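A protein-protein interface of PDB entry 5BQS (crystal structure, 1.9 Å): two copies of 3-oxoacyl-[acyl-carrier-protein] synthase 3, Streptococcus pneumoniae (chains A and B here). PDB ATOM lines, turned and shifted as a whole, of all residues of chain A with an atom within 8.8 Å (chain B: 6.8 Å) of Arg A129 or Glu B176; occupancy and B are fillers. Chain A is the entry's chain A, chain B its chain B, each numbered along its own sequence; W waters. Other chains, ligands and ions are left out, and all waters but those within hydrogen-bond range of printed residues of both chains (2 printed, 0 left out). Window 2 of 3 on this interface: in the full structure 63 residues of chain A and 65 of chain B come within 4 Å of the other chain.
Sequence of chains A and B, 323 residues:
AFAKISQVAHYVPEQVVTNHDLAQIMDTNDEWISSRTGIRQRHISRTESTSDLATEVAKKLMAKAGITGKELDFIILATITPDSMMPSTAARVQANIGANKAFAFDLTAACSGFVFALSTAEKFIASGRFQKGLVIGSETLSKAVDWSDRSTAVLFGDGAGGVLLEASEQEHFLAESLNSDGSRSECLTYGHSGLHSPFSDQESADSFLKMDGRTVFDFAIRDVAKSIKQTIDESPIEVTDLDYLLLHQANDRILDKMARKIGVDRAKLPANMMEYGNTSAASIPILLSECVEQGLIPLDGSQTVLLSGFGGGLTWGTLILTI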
ATOM      1  N   ALA A   1       6.527  24.523  15.078  1.00  0.00           N
ATOM      2  CA  ALA A   1       7.232  25.773  14.786  1.00  0.00           C
ATOM      3  C   ALA A   1       7.050  26.183  13.327  1.00  0.00           C
ATOM      4  O   ALA A   1       6.584  25.371  12.524  1.00  0.00           O
ATOM      5  CB  ALA A   1       8.711  25.618  15.101  1.00  0.00           C
ATOM      6  N   ASP A  73      21.824  23.910  12.607  1.00  0.00           N
ATOM      7  CA  ASP A  73      21.203  22.591  12.869  1.00  0.00           C
ATOM      8  C   ASP A  73      21.293  21.639  11.673  1.00  0.00           C
ATOM      9  O   ASP A  73      21.297  20.417  11.837  1.00  0.00           O
ATOM     10  CB  ASP A  73      19.733  22.767  13.310  1.00  0.00           C
ATOM     11  CG  ASP A  73      19.620  23.552  14.609  1.00  0.00           C
ATOM     12  OD1 ASP A  73      20.135  23.077  15.628  1.00  0.00           O
ATOM     13  OD2 ASP A  73      19.052  24.655  14.587  1.00  0.00           O
ATOM     14  N   PHE A  74      21.336  22.191  10.473  1.00  0.00           N
ATOM     15  CA  PHE A  74      21.409  21.398   9.249  1.00  0.00           C
ATOM     16  C   PHE A  74      21.956  22.194   8.089  1.00  0.00           C
ATOM     17  O   PHE A  74      21.928  23.431   8.095  1.00  0.00           O
ATOM     18  CB  PHE A  74      20.022  20.783   8.866  1.00  0.00           C
ATOM     19  CG  PHE A  74      18.907  21.779   8.658  1.00  0.00           C
ATOM     20  CD1 PHE A  74      18.739  22.416   7.430  1.00  0.00           C
ATOM     21  CD2 PHE A  74      18.028  22.093   9.694  1.00  0.00           C
ATOM     22  CE1 PHE A  74      17.725  23.360   7.245  1.00  0.00           C
ATOM     23  CE2 PHE A  74      17.019  23.046   9.509  1.00  0.00           C
ATOM     24  CZ  PHE A  74      16.866  23.664   8.278  1.00  0.00           C
ATOM     25  N   LYS A 101      27.521  20.786  14.999  1.00  0.00           N
ATOM     26  CA  LYS A 101      26.250  20.238  15.501  1.00  0.00           C
ATOM     27  C   LYS A 101      25.223  19.932  14.368  1.00  0.00           C
ATOM     28  O   LYS A 101      24.186  19.314  14.630  1.00  0.00           O
ATOM     29  CB  LYS A 101      25.642  21.120  16.622  1.00  0.00           C
ATOM     30  CG  LYS A 101      24.789  22.299  16.174  1.00  0.00           C
ATOM     31  CD  LYS A 101      23.968  22.907  17.306  1.00  0.00           C
ATOM     32  CE  LYS A 101      23.120  24.050  16.782  1.00  0.00           C
ATOM     33  NZ  LYS A 101      22.179  24.592  17.806  1.00  0.00           N
ATOM     34  N   PHE A 103      23.553  18.314  10.753  1.00  0.00           N
ATOM     35  CA  PHE A 103      23.530  17.104   9.937  1.00  0.00           C
ATOM     36  C   PHE A 103      23.531  17.664   8.518  1.00  0.00           C
ATOM     37  O   PHE A 103      23.022  18.775   8.299  1.00  0.00           O
ATOM     38  CB  PHE A 103      22.324  16.173  10.207  1.00  0.00           C
ATOM     39  CG  PHE A 103      20.949  16.753   9.991  1.00  0.00           C
ATOM     40  CD1 PHE A 103      20.359  16.731   8.733  1.00  0.00           C
ATOM     41  CD2 PHE A 103      20.215  17.261  11.063  1.00  0.00           C
ATOM     42  CE1 PHE A 103      19.078  17.239   8.536  1.00  0.00           C
ATOM     43  CE2 PHE A 103      18.923  17.748  10.870  1.00  0.00           C
ATOM     44  CZ  PHE A 103      18.366  17.737   9.610  1.00  0.00           C
ATOM     45  N   LYS A 123      10.034  21.541   6.731  1.00  0.00           N
ATOM     46  CA  LYS A 123       9.449  20.429   7.495  1.00  0.00           C
ATOM     47  C   LYS A 123      10.304  20.110   8.723  1.00  0.00           C
ATOM     48  O   LYS A 123       9.763  19.738   9.763  1.00  0.00           O
ATOM     49  CB  LYS A 123       9.293  19.149   6.637  1.00  0.00           C
ATOM     50  CG  LYS A 123       8.423  19.147   5.367  1.00  0.00           C
ATOM     51  CD  LYS A 123       7.198  20.017   5.374  1.00  0.00           C
ATOM     52  CE  LYS A 123       6.556  20.093   4.031  1.00  0.00           C
ATOM     53  NZ  LYS A 123       6.838  21.390   3.344  1.00  0.00           N
ATOM     54  N   PHE A 124      11.634  20.245   8.605  1.00  0.00           N
ATOM     55  CA  PHE A 124      12.551  19.997   9.726  1.00  0.00           C
ATOM     56  C   PHE A 124      12.405  21.100  10.780  1.00  0.00           C
ATOM     57  O   PHE A 124      12.392  20.800  11.971  1.00  0.00           O
ATOM     58  CB  PHE A 124      14.009  19.868   9.261  1.00  0.00           C
ATOM     59  CG  PHE A 124      14.372  18.475   8.805  1.00  0.00           C
ATOM     60  CD1 PHE A 124      14.725  17.489   9.728  1.00  0.00           C
ATOM     61  CD2 PHE A 124      14.313  18.130   7.461  1.00  0.00           C
ATOM     62  CE1 PHE A 124      15.021  16.187   9.309  1.00  0.00           C
ATOM     63  CE2 PHE A 124      14.615  16.831   7.045  1.00  0.00           C
ATOM     64  CZ  PHE A 124      14.978  15.873   7.972  1.00  0.00           C
ATOM     65  N   ILE A 125      12.275  22.365  10.344  1.00  0.00           N
ATOM     66  CA  ILE A 125      12.092  23.466  11.293  1.00  0.00           C
ATOM     67  C   ILE A 125      10.704  23.341  11.942  1.00  0.00           C
ATOM     68  O   ILE A 125      10.598  23.523  13.143  1.00  0.00           O
ATOM     69  CB  ILE A 125      12.392  24.862  10.673  1.00  0.00           C
ATOM     70  CG1 ILE A 125      13.901  24.955  10.348  1.00  0.00           C
ATOM     71  CG2 ILE A 125      11.941  26.026  11.621  1.00  0.00           C
ATOM     72  CD1 ILE A 125      14.394  26.207   9.763  1.00  0.00           C
ATOM     73  N   ALA A 126       9.667  22.971  11.154  1.00  0.00           N
ATOM     74  CA  ALA A 126       8.288  22.772  11.625  1.00  0.00           C
ATOM     75  C   ALA A 126       8.183  21.808  12.797  1.00  0.00           C
ATOM     76  O   ALA A 126       7.302  21.981  13.634  1.00  0.00           O
ATOM     77  CB  ALA A 126       7.393  22.315  10.478  1.00  0.00           C
ATOM     78  N   SER A 127       9.105  20.820  12.888  1.00  0.00           N
ATOM     79  CA  SER A 127       9.183  19.836  13.978  1.00  0.00           C
ATOM     80  C   SER A 127       9.490  20.472  15.341  1.00  0.00           C
ATOM     81  O   SER A 127       9.193  19.856  16.366  1.00  0.00           O
ATOM     82  CB  SER A 127      10.230  18.772  13.672  1.00  0.00           C
ATOM     83  OG  SER A 127      11.532  19.245  13.958  1.00  0.00           O
ATOM     84  N   GLY A 128      10.122  21.654  15.341  1.00  0.00           N
ATOM     85  CA  GLY A 128      10.478  22.363  16.568  1.00  0.00           C
ATOM     86  C   GLY A 128      11.761  21.882  17.225  1.00  0.00           C
ATOM     87  O   GLY A 128      12.118  22.359  18.301  1.00  0.00           O
ATOM     88  N   ARG A 129      12.462  20.939  16.589  1.00  0.00           N
ATOM     89  CA  ARG A 129      13.733  20.410  17.076  1.00  0.00           C
ATOM     90  C   ARG A 129      14.873  21.289  16.564  1.00  0.00           C
ATOM     91  O   ARG A 129      15.932  21.361  17.197  1.00  0.00           O
ATOM     92  CB  ARG A 129      13.937  18.973  16.560  1.00  0.00           C
ATOM     93  CG  ARG A 129      13.725  17.902  17.626  1.00  0.00           C
ATOM     94  CD  ARG A 129      13.835  16.483  17.074  1.00  0.00           C
ATOM     95  NE  ARG A 129      15.163  16.180  16.529  1.00  0.00           N
ATOM     96  CZ  ARG A 129      16.181  15.695  17.237  1.00  0.00           C
ATOM     97  NH1 ARG A 129      16.039  15.445  18.533  1.00  0.00           N
ATOM     98  NH2 ARG A 129      17.346  15.454  16.653  1.00  0.00           N
ATOM     99  N   PHE A 130      14.663  21.940  15.401  1.00  0.00           N
ATOM    100  CA  PHE A 130      15.684  22.744  14.739  1.00  0.00           C
ATOM    101  C   PHE A 130      15.294  24.216  14.632  1.00  0.00           C
ATOM    102  O   PHE A 130      14.112  24.530  14.443  1.00  0.00           O
ATOM    103  CB  PHE A 130      16.042  22.111  13.383  1.00  0.00           C
ATOM    104  CG  PHE A 130      16.231  20.609  13.497  1.00  0.00           C
ATOM    105  CD1 PHE A 130      17.330  20.077  14.164  1.00  0.00           C
ATOM    106  CD2 PHE A 130      15.271  19.732  13.009  1.00  0.00           C
ATOM    107  CE1 PHE A 130      17.482  18.694  14.302  1.00  0.00           C
ATOM    108  CE2 PHE A 130      15.417  18.353  13.165  1.00  0.00           C
ATOM    109  CZ  PHE A 130      16.531  17.844  13.791  1.00  0.00           C
ATOM    110  N   GLN A 131      16.290  25.112  14.829  1.00  0.00           N
ATOM    111  CA  GLN A 131      16.144  26.568  14.844  1.00  0.00           C
ATOM    112  C   GLN A 131      16.729  27.291  13.638  1.00  0.00           C
ATOM    113  O   GLN A 131      16.264  28.383  13.331  1.00  0.00           O
ATOM    114  CB  GLN A 131      16.852  27.158  16.078  1.00  0.00           C
ATOM    115  CG  GLN A 131      16.247  26.819  17.430  1.00  0.00           C
ATOM    116  CD  GLN A 131      17.302  26.989  18.488  1.00  0.00           C
ATOM    117  OE1 GLN A 131      17.722  28.111  18.808  1.00  0.00           O
ATOM    118  NE2 GLN A 131      17.800  25.873  19.009  1.00  0.00           N
ATOM    119  N   LYS A 132      17.842  26.791  13.076  1.00  0.00           N
ATOM    120  CA  LYS A 132      18.593  27.430  11.979  1.00  0.00           C
ATOM    121  C   LYS A 132      19.173  26.363  11.055  1.00  0.00           C
ATOM    122  O   LYS A 132      19.702  25.372  11.537  1.00  0.00           O
ATOM    123  CB  LYS A 132      19.817  28.195  12.536  1.00  0.00           C
ATOM    124  CG  LYS A 132      19.536  29.341  13.486  1.00  0.00           C
ATOM    125  CD  LYS A 132      20.826  29.924  14.036  1.00  0.00           C
ATOM    126  CE  LYS A 132      20.582  30.771  15.272  1.00  0.00           C
ATOM    127  NZ  LYS A 132      19.632  31.888  15.017  1.00  0.00           N
ATOM    128  N   ALA A 167      13.763  29.456  12.664  1.00  0.00           N
ATOM    129  CA  ALA A 167      12.495  29.278  13.357  1.00  0.00           C
ATOM    130  C   ALA A 167      11.851  30.645  13.598  1.00  0.00           C
ATOM    131  O   ALA A 167      12.551  31.639  13.822  1.00  0.00           O
ATOM    132  CB  ALA A 167      12.708  28.548  14.676  1.00  0.00           C
ATOM    133  N   VAL B 115      18.159   6.058   6.905  1.00  0.00           N
ATOM    134  CA  VAL B 115      17.693   6.671   8.145  1.00  0.00           C
ATOM    135  C   VAL B 115      17.365   8.177   7.926  1.00  0.00           C
ATOM    136  O   VAL B 115      16.304   8.640   8.375  1.00  0.00           O
ATOM    137  CB  VAL B 115      18.703   6.416   9.281  1.00  0.00           C
ATOM    138  CG1 VAL B 115      18.411   7.304  10.483  1.00  0.00           C
ATOM    139  CG2 VAL B 115      18.710   4.938   9.678  1.00  0.00           C
ATOM    140  N   LEU B 118      14.177   8.379   5.931  1.00  0.00           N
ATOM    141  CA  LEU B 118      13.023   7.977   6.733  1.00  0.00           C
ATOM    142  C   LEU B 118      12.617   9.121   7.655  1.00  0.00           C
ATOM    143  O   LEU B 118      11.429   9.414   7.766  1.00  0.00           O
ATOM    144  CB  LEU B 118      13.342   6.682   7.516  1.00  0.00           C
ATOM    145  CG  LEU B 118      12.169   6.010   8.256  1.00  0.00           C
ATOM    146  CD1 LEU B 118      11.074   5.573   7.277  1.00  0.00           C
ATOM    147  CD2 LEU B 118      12.669   4.816   9.052  1.00  0.00           C
ATOM    148  N   SER B 119      13.605   9.822   8.239  1.00  0.00           N
ATOM    149  CA  SER B 119      13.381  11.006   9.064  1.00  0.00           C
ATOM    150  C   SER B 119      12.741  12.119   8.212  1.00  0.00           C
ATOM    151  O   SER B 119      11.767  12.737   8.638  1.00  0.00           O
ATOM    152  CB  SER B 119      14.691  11.491   9.669  1.00  0.00           C
ATOM    153  OG  SER B 119      14.517  12.759  10.280  1.00  0.00           O
ATOM    154  N   THR B 120      13.262  12.330   6.987  1.00  0.00           N
ATOM    155  CA  THR B 120      12.757  13.360   6.058  1.00  0.00           C
ATOM    156  C   THR B 120      11.313  13.069   5.721  1.00  0.00           C
ATOM    157  O   THR B 120      10.472  13.973   5.786  1.00  0.00           O
ATOM    158  CB  THR B 120      13.609  13.399   4.770  1.00  0.00           C
ATOM    159  OG1 THR B 120      14.933  13.786   5.116  1.00  0.00           O
ATOM    160  CG2 THR B 120      13.054  14.388   3.730  1.00  0.00           C
ATOM    161  N   GLU B 122       9.167  11.330   7.322  1.00  0.00           N
ATOM    162  CA  GLU B 122       8.357  11.504   8.527  1.00  0.00           C
ATOM    163  C   GLU B 122       7.962  12.984   8.708  1.00  0.00           C
ATOM    164  O   GLU B 122       6.825  13.259   9.086  1.00  0.00           O
ATOM    165  CB  GLU B 122       9.088  10.891   9.742  1.00  0.00           C
ATOM    166  CG  GLU B 122       8.322  10.927  11.043  1.00  0.00           C
ATOM    167  CD  GLU B 122       8.717  12.108  11.899  1.00  0.00           C
ATOM    168  OE1 GLU B 122       9.934  12.365  12.044  1.00  0.00           O
ATOM    169  OE2 GLU B 122       7.805  12.767  12.439  1.00  0.00           O
ATOM    170  N   LYS B 123       8.870  13.938   8.378  1.00  0.00           N
ATOM    171  CA  LYS B 123       8.588  15.369   8.463  1.00  0.00           C
ATOM    172  C   LYS B 123       7.510  15.790   7.461  1.00  0.00           C
ATOM    173  O   LYS B 123       6.724  16.702   7.747  1.00  0.00           O
ATOM    174  CB  LYS B 123       9.862  16.204   8.235  1.00  0.00           C
ATOM    175  CG  LYS B 123      10.589  16.520   9.534  1.00  0.00           C
ATOM    176  CD  LYS B 123      11.530  15.516   9.849  1.00  0.00           C
ATOM    177  CE  LYS B 123      11.953  15.432  11.294  1.00  0.00           C
ATOM    178  NZ  LYS B 123      12.159  13.999  11.593  1.00  0.00           N
ATOM    179  N   PHE B 173       7.430   7.302  15.931  1.00  0.00           N
ATOM    180  CA  PHE B 173       8.770   7.883  15.967  1.00  0.00           C
ATOM    181  C   PHE B 173       9.019   8.457  17.358  1.00  0.00           C
ATOM    182  O   PHE B 173       8.472   9.491  17.728  1.00  0.00           O
ATOM    183  CB  PHE B 173       8.955   8.903  14.823  1.00  0.00           C
ATOM    184  CG  PHE B 173       9.128   8.261  13.459  1.00  0.00           C
ATOM    185  CD1 PHE B 173       8.073   7.599  12.840  1.00  0.00           C
ATOM    186  CD2 PHE B 173      10.330   8.354  12.778  1.00  0.00           C
ATOM    187  CE1 PHE B 173       8.241   6.984  11.596  1.00  0.00           C
ATOM    188  CE2 PHE B 173      10.490   7.758  11.522  1.00  0.00           C
ATOM    189  CZ  PHE B 173       9.443   7.082  10.938  1.00  0.00           C
ATOM    190  N   LEU B 174       9.813   7.735  18.158  1.00  0.00           N
ATOM    191  CA  LEU B 174      10.069   8.104  19.549  1.00  0.00           C
ATOM    192  C   LEU B 174      11.278   8.997  19.764  1.00  0.00           C
ATOM    193  O   LEU B 174      11.271   9.792  20.703  1.00  0.00           O
ATOM    194  CB  LEU B 174      10.162   6.854  20.426  1.00  0.00           C
ATOM    195  CG  LEU B 174       9.026   5.848  20.288  1.00  0.00           C
ATOM    196  CD1 LEU B 174       9.290   4.630  21.147  1.00  0.00           C
ATOM    197  CD2 LEU B 174       7.668   6.467  20.640  1.00  0.00           C
ATOM    198  N   ALA B 175      12.310   8.879  18.908  1.00  0.00           N
ATOM    199  CA  ALA B 175      13.538   9.664  19.043  1.00  0.00           C
ATOM    200  C   ALA B 175      14.334   9.639  17.762  1.00  0.00           C
ATOM    201  O   ALA B 175      14.234   8.693  16.993  1.00  0.00           O
ATOM    202  CB  ALA B 175      14.388   9.105  20.178  1.00  0.00           C
ATOM    203  N   GLU B 176      15.148  10.672  17.550  1.00  0.00           N
ATOM    204  CA  GLU B 176      16.017  10.760  16.381  1.00  0.00           C
ATOM    205  C   GLU B 176      17.253  11.573  16.673  1.00  0.00           C
ATOM    206  O   GLU B 176      17.201  12.523  17.452  1.00  0.00           O
ATOM    207  CB  GLU B 176      15.276  11.285  15.146  1.00  0.00           C
ATOM    208  CG  GLU B 176      15.140  12.791  15.064  1.00  0.00           C
ATOM    209  CD  GLU B 176      14.556  13.315  13.772  1.00  0.00           C
ATOM    210  OE1 GLU B 176      14.406  14.553  13.643  1.00  0.00           O
ATOM    211  OE2 GLU B 176      14.211  12.487  12.902  1.00  0.00           O
ATOM    212  N   SER B 177      18.366  11.188  16.046  1.00  0.00           N
ATOM    213  CA  SER B 177      19.623  11.906  16.151  1.00  0.00           C
ATOM    214  C   SER B 177      20.280  11.758  14.789  1.00  0.00           C
ATOM    215  O   SER B 177      20.723  10.666  14.442  1.00  0.00           O
ATOM    216  CB  SER B 177      20.511  11.309  17.241  1.00  0.00           C
ATOM    217  OG  SER B 177      21.711  12.048  17.385  1.00  0.00           O
ATOM    218  N   LEU B 178      20.277  12.835  13.997  1.00  0.00           N
ATOM    219  CA  LEU B 178      20.903  12.870  12.680  1.00  0.00           C
ATOM    220  C   LEU B 178      22.159  13.707  12.838  1.00  0.00           C
ATOM    221  O   LEU B 178      22.123  14.769  13.458  1.00  0.00           O
ATOM    222  CB  LEU B 178      19.967  13.472  11.622  1.00  0.00           C
ATOM    223  CG  LEU B 178      18.554  12.911  11.512  1.00  0.00           C
ATOM    224  CD1 LEU B 178      17.797  13.636  10.395  1.00  0.00           C
ATOM    225  CD2 LEU B 178      18.560  11.412  11.188  1.00  0.00           C
ATOM    226  N   ASN B 179      23.290  13.174  12.361  1.00  0.00           N
ATOM    227  CA  ASN B 179      24.593  13.756  12.572  1.00  0.00           C
ATOM    228  C   ASN B 179      25.465  13.606  11.353  1.00  0.00           C
ATOM    229  O   ASN B 179      25.271  12.705  10.537  1.00  0.00           O
ATOM    230  CB  ASN B 179      25.299  13.058  13.745  1.00  0.00           C
ATOM    231  CG  ASN B 179      24.511  12.992  15.028  1.00  0.00           C
ATOM    232  OD1 ASN B 179      24.510  13.917  15.825  1.00  0.00           O
ATOM    233  ND2 ASN B 179      23.765  11.924  15.209  1.00  0.00           N
ATOM    234  N   THR B 231      21.210   8.676  22.321  1.00  0.00           N
ATOM    235  CA  THR B 231      19.869   8.743  21.715  1.00  0.00           C
ATOM    236  C   THR B 231      18.872   8.001  22.615  1.00  0.00           C
ATOM    237  O   THR B 231      17.822   8.563  22.944  1.00  0.00           O
ATOM    238  CB  THR B 231      19.878   8.190  20.282  1.00  0.00           C
ATOM    239  OG1 THR B 231      20.866   8.905  19.529  1.00  0.00           O
ATOM    240  CG2 THR B 231      18.488   8.298  19.583  1.00  0.00           C
ATOM    241  N   GLU B 234      18.306  10.029  25.939  1.00  0.00           N
ATOM    242  CA  GLU B 234      17.438  11.179  25.709  1.00  0.00           C
ATOM    243  C   GLU B 234      16.008  10.796  25.297  1.00  0.00           C
ATOM    244  O   GLU B 234      15.097  11.604  25.461  1.00  0.00           O
ATOM    245  CB  GLU B 234      18.076  12.130  24.693  1.00  0.00           C
ATOM    246  CG  GLU B 234      19.352  12.771  25.208  1.00  0.00           C
ATOM    247  CD  GLU B 234      20.104  13.702  24.270  1.00  0.00           C
ATOM    248  OE1 GLU B 234      19.573  14.052  23.191  1.00  0.00           O
ATOM    249  OE2 GLU B 234      21.238  14.090  24.633  1.00  0.00           O
ATOM    250  N   SER B 235      15.810   9.569  24.777  1.00  0.00           N
ATOM    251  CA  SER B 235      14.497   9.066  24.357  1.00  0.00           C
ATOM    252  C   SER B 235      13.597   8.739  25.581  1.00  0.00           C
ATOM    253  O   SER B 235      14.117   8.570  26.684  1.00  0.00           O
ATOM    254  CB  SER B 235      14.665   7.820  23.494  1.00  0.00           C
ATOM    255  OG  SER B 235      14.920   6.657  24.265  1.00  0.00           O
ATOM    256  N   GLY B 317      23.029   8.343  11.718  1.00  0.00           N
ATOM    257  CA  GLY B 317      21.659   8.659  12.081  1.00  0.00           C
ATOM    258  C   GLY B 317      21.041   7.533  12.866  1.00  0.00           C
ATOM    259  O   GLY B 317      21.214   6.369  12.508  1.00  0.00           O
ATOM    260  N   THR B 318      20.322   7.880  13.931  1.00  0.00           N
ATOM    261  CA  THR B 318      19.678   6.931  14.833  1.00  0.00           C
ATOM    262  C   THR B 318      18.213   7.292  14.988  1.00  0.00           C
ATOM    263  O   THR B 318      17.869   8.440  15.253  1.00  0.00           O
ATOM    264  CB  THR B 318      20.428   6.851  16.180  1.00  0.00           C
ATOM    265  OG1 THR B 318      21.793   6.563  15.918  1.00  0.00           O
ATOM    266  CG2 THR B 318      19.875   5.771  17.108  1.00  0.00           C
ATOM    267  N   LEU B 319      17.355   6.297  14.801  1.00  0.00           N
ATOM    268  CA  LEU B 319      15.926   6.449  14.985  1.00  0.00           C
ATOM    269  C   LEU B 319      15.464   5.407  15.983  1.00  0.00           C
ATOM    270  O   LEU B 319      15.904   4.258  15.926  1.00  0.00           O
ATOM    271  CB  LEU B 319      15.165   6.266  13.665  1.00  0.00           C
ATOM    272  CG  LEU B 319      15.363   7.332  12.582  1.00  0.00           C
ATOM    273  CD1 LEU B 319      14.740   6.895  11.259  1.00  0.00           C
ATOM    274  CD2 LEU B 319      14.747   8.642  12.980  1.00  0.00           C
ATOM    275  N   ILE B 320      14.589   5.807  16.895  1.00  0.00           N
ATOM    276  CA  ILE B 320      13.958   4.872  17.830  1.00  0.00           C
ATOM    277  C   ILE B 320      12.489   4.959  17.514  1.00  0.00           C
ATOM    278  O   ILE B 320      11.922   6.052  17.477  1.00  0.00           O
ATOM    279  CB  ILE B 320      14.290   5.085  19.322  1.00  0.00           C
ATOM    280  CG1 ILE B 320      15.804   4.978  19.564  1.00  0.00           C
ATOM    281  CG2 ILE B 320      13.521   4.072  20.213  1.00  0.00           C
ATOM    282  CD1 ILE B 320      16.285   5.445  20.976  1.00  0.00           C
HETATM  283  O   HOH W   1       6.542  18.840   9.438  1.00  0.00           O
HETATM  284  O   HOH W   2      14.480  12.950  19.337  1.00  0.00           O
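Water W1 bridges the backbone carbonyl oxygen (O) of Lys B123 and the backbone carbonyl oxygen (O) of Lys A123. Water W2 lies within hydrogen-bond range of N of Glu B176 (3.0 Å) and NH1 of Arg A129 (3.0 Å).
Among the printed residues, pairs that only touch across the chains: Lys A123 with Lys B123, Phe A124 with Thr B120, Phe A103 with Leu B178, Phe A124 with Lys B123, Phe A124 with Ser B119, Phe A103 with Asn B179, Phe A130 with Glu B176 and Phe A124 with Leu B178.
The backbone NH (N) of Phe A103 sits at hydrogen-bond distance from the backbone carbonyl oxygen (O) of Asp A73, at 3.3 Å. The side-chain carboxylate (OE2) of Glu B176 sits at hydrogen-bond distance from the side-chain hydroxyl (OG) of Ser B119 (2.7 Å). The side-chain hydroxyl (OG) of Ser A127 lies close to the backbone NH (N) of Arg A129, at 3.3 Å. The side-chain amino group (NZ) of Lys B123 lies within salt-bridge range of the side-chain carboxylate (OE2) of Glu B176. OG of Ser A127 is in hydrogen-bond range of O of Phe A124. The side-chain amino group (NZ) of Lys B123 is in salt-bridge range of the side-chain carboxylate (OE1) of Glu B122.
Arg A129 touches just one residue of chain B: Glu B176 (3.0 Å). Of chain A, only Arg A129 (3.0 Å) and Phe A130 (3.9 Å) come within 4 Å of Glu B176. No residue of chain A comes within 4 Å of Ala B175. No residue of chain A comes within 4 Å of Ser B177. Of the printed residues of chain A, Lys B123 touches Lys A123 (3.3 Å) and Phe A124 (3.6 Å). Of the printed residues of chain B, Phe A130 touches Glu B176 (3.9 Å). The nearest printed residue of chain B that does not touch Phe A124 is Glu B176 (4.7 Å).
Of the 20 printed residues of chain B, 6 touch a printed residue of chain A. Of the 16 printed residues of chain A, 5 touch a printed residue of chain B. Hydrophobic or aromatic side chains of chain A within 4 Å of the printed part of chain B: Phe A103, Phe A124 and Phe A130. Among the printed residues, Asp or Glu carboxylates within 4 Å of a Lys or Arg side-chain nitrogen of the other chain: Arg A129 with Glu B176.
Lys B123 touches its own counterpart, Lys A123.
NE of Arg A129 lies within salt-bridge range of OE1 of Glu B176 (3.4 Å).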
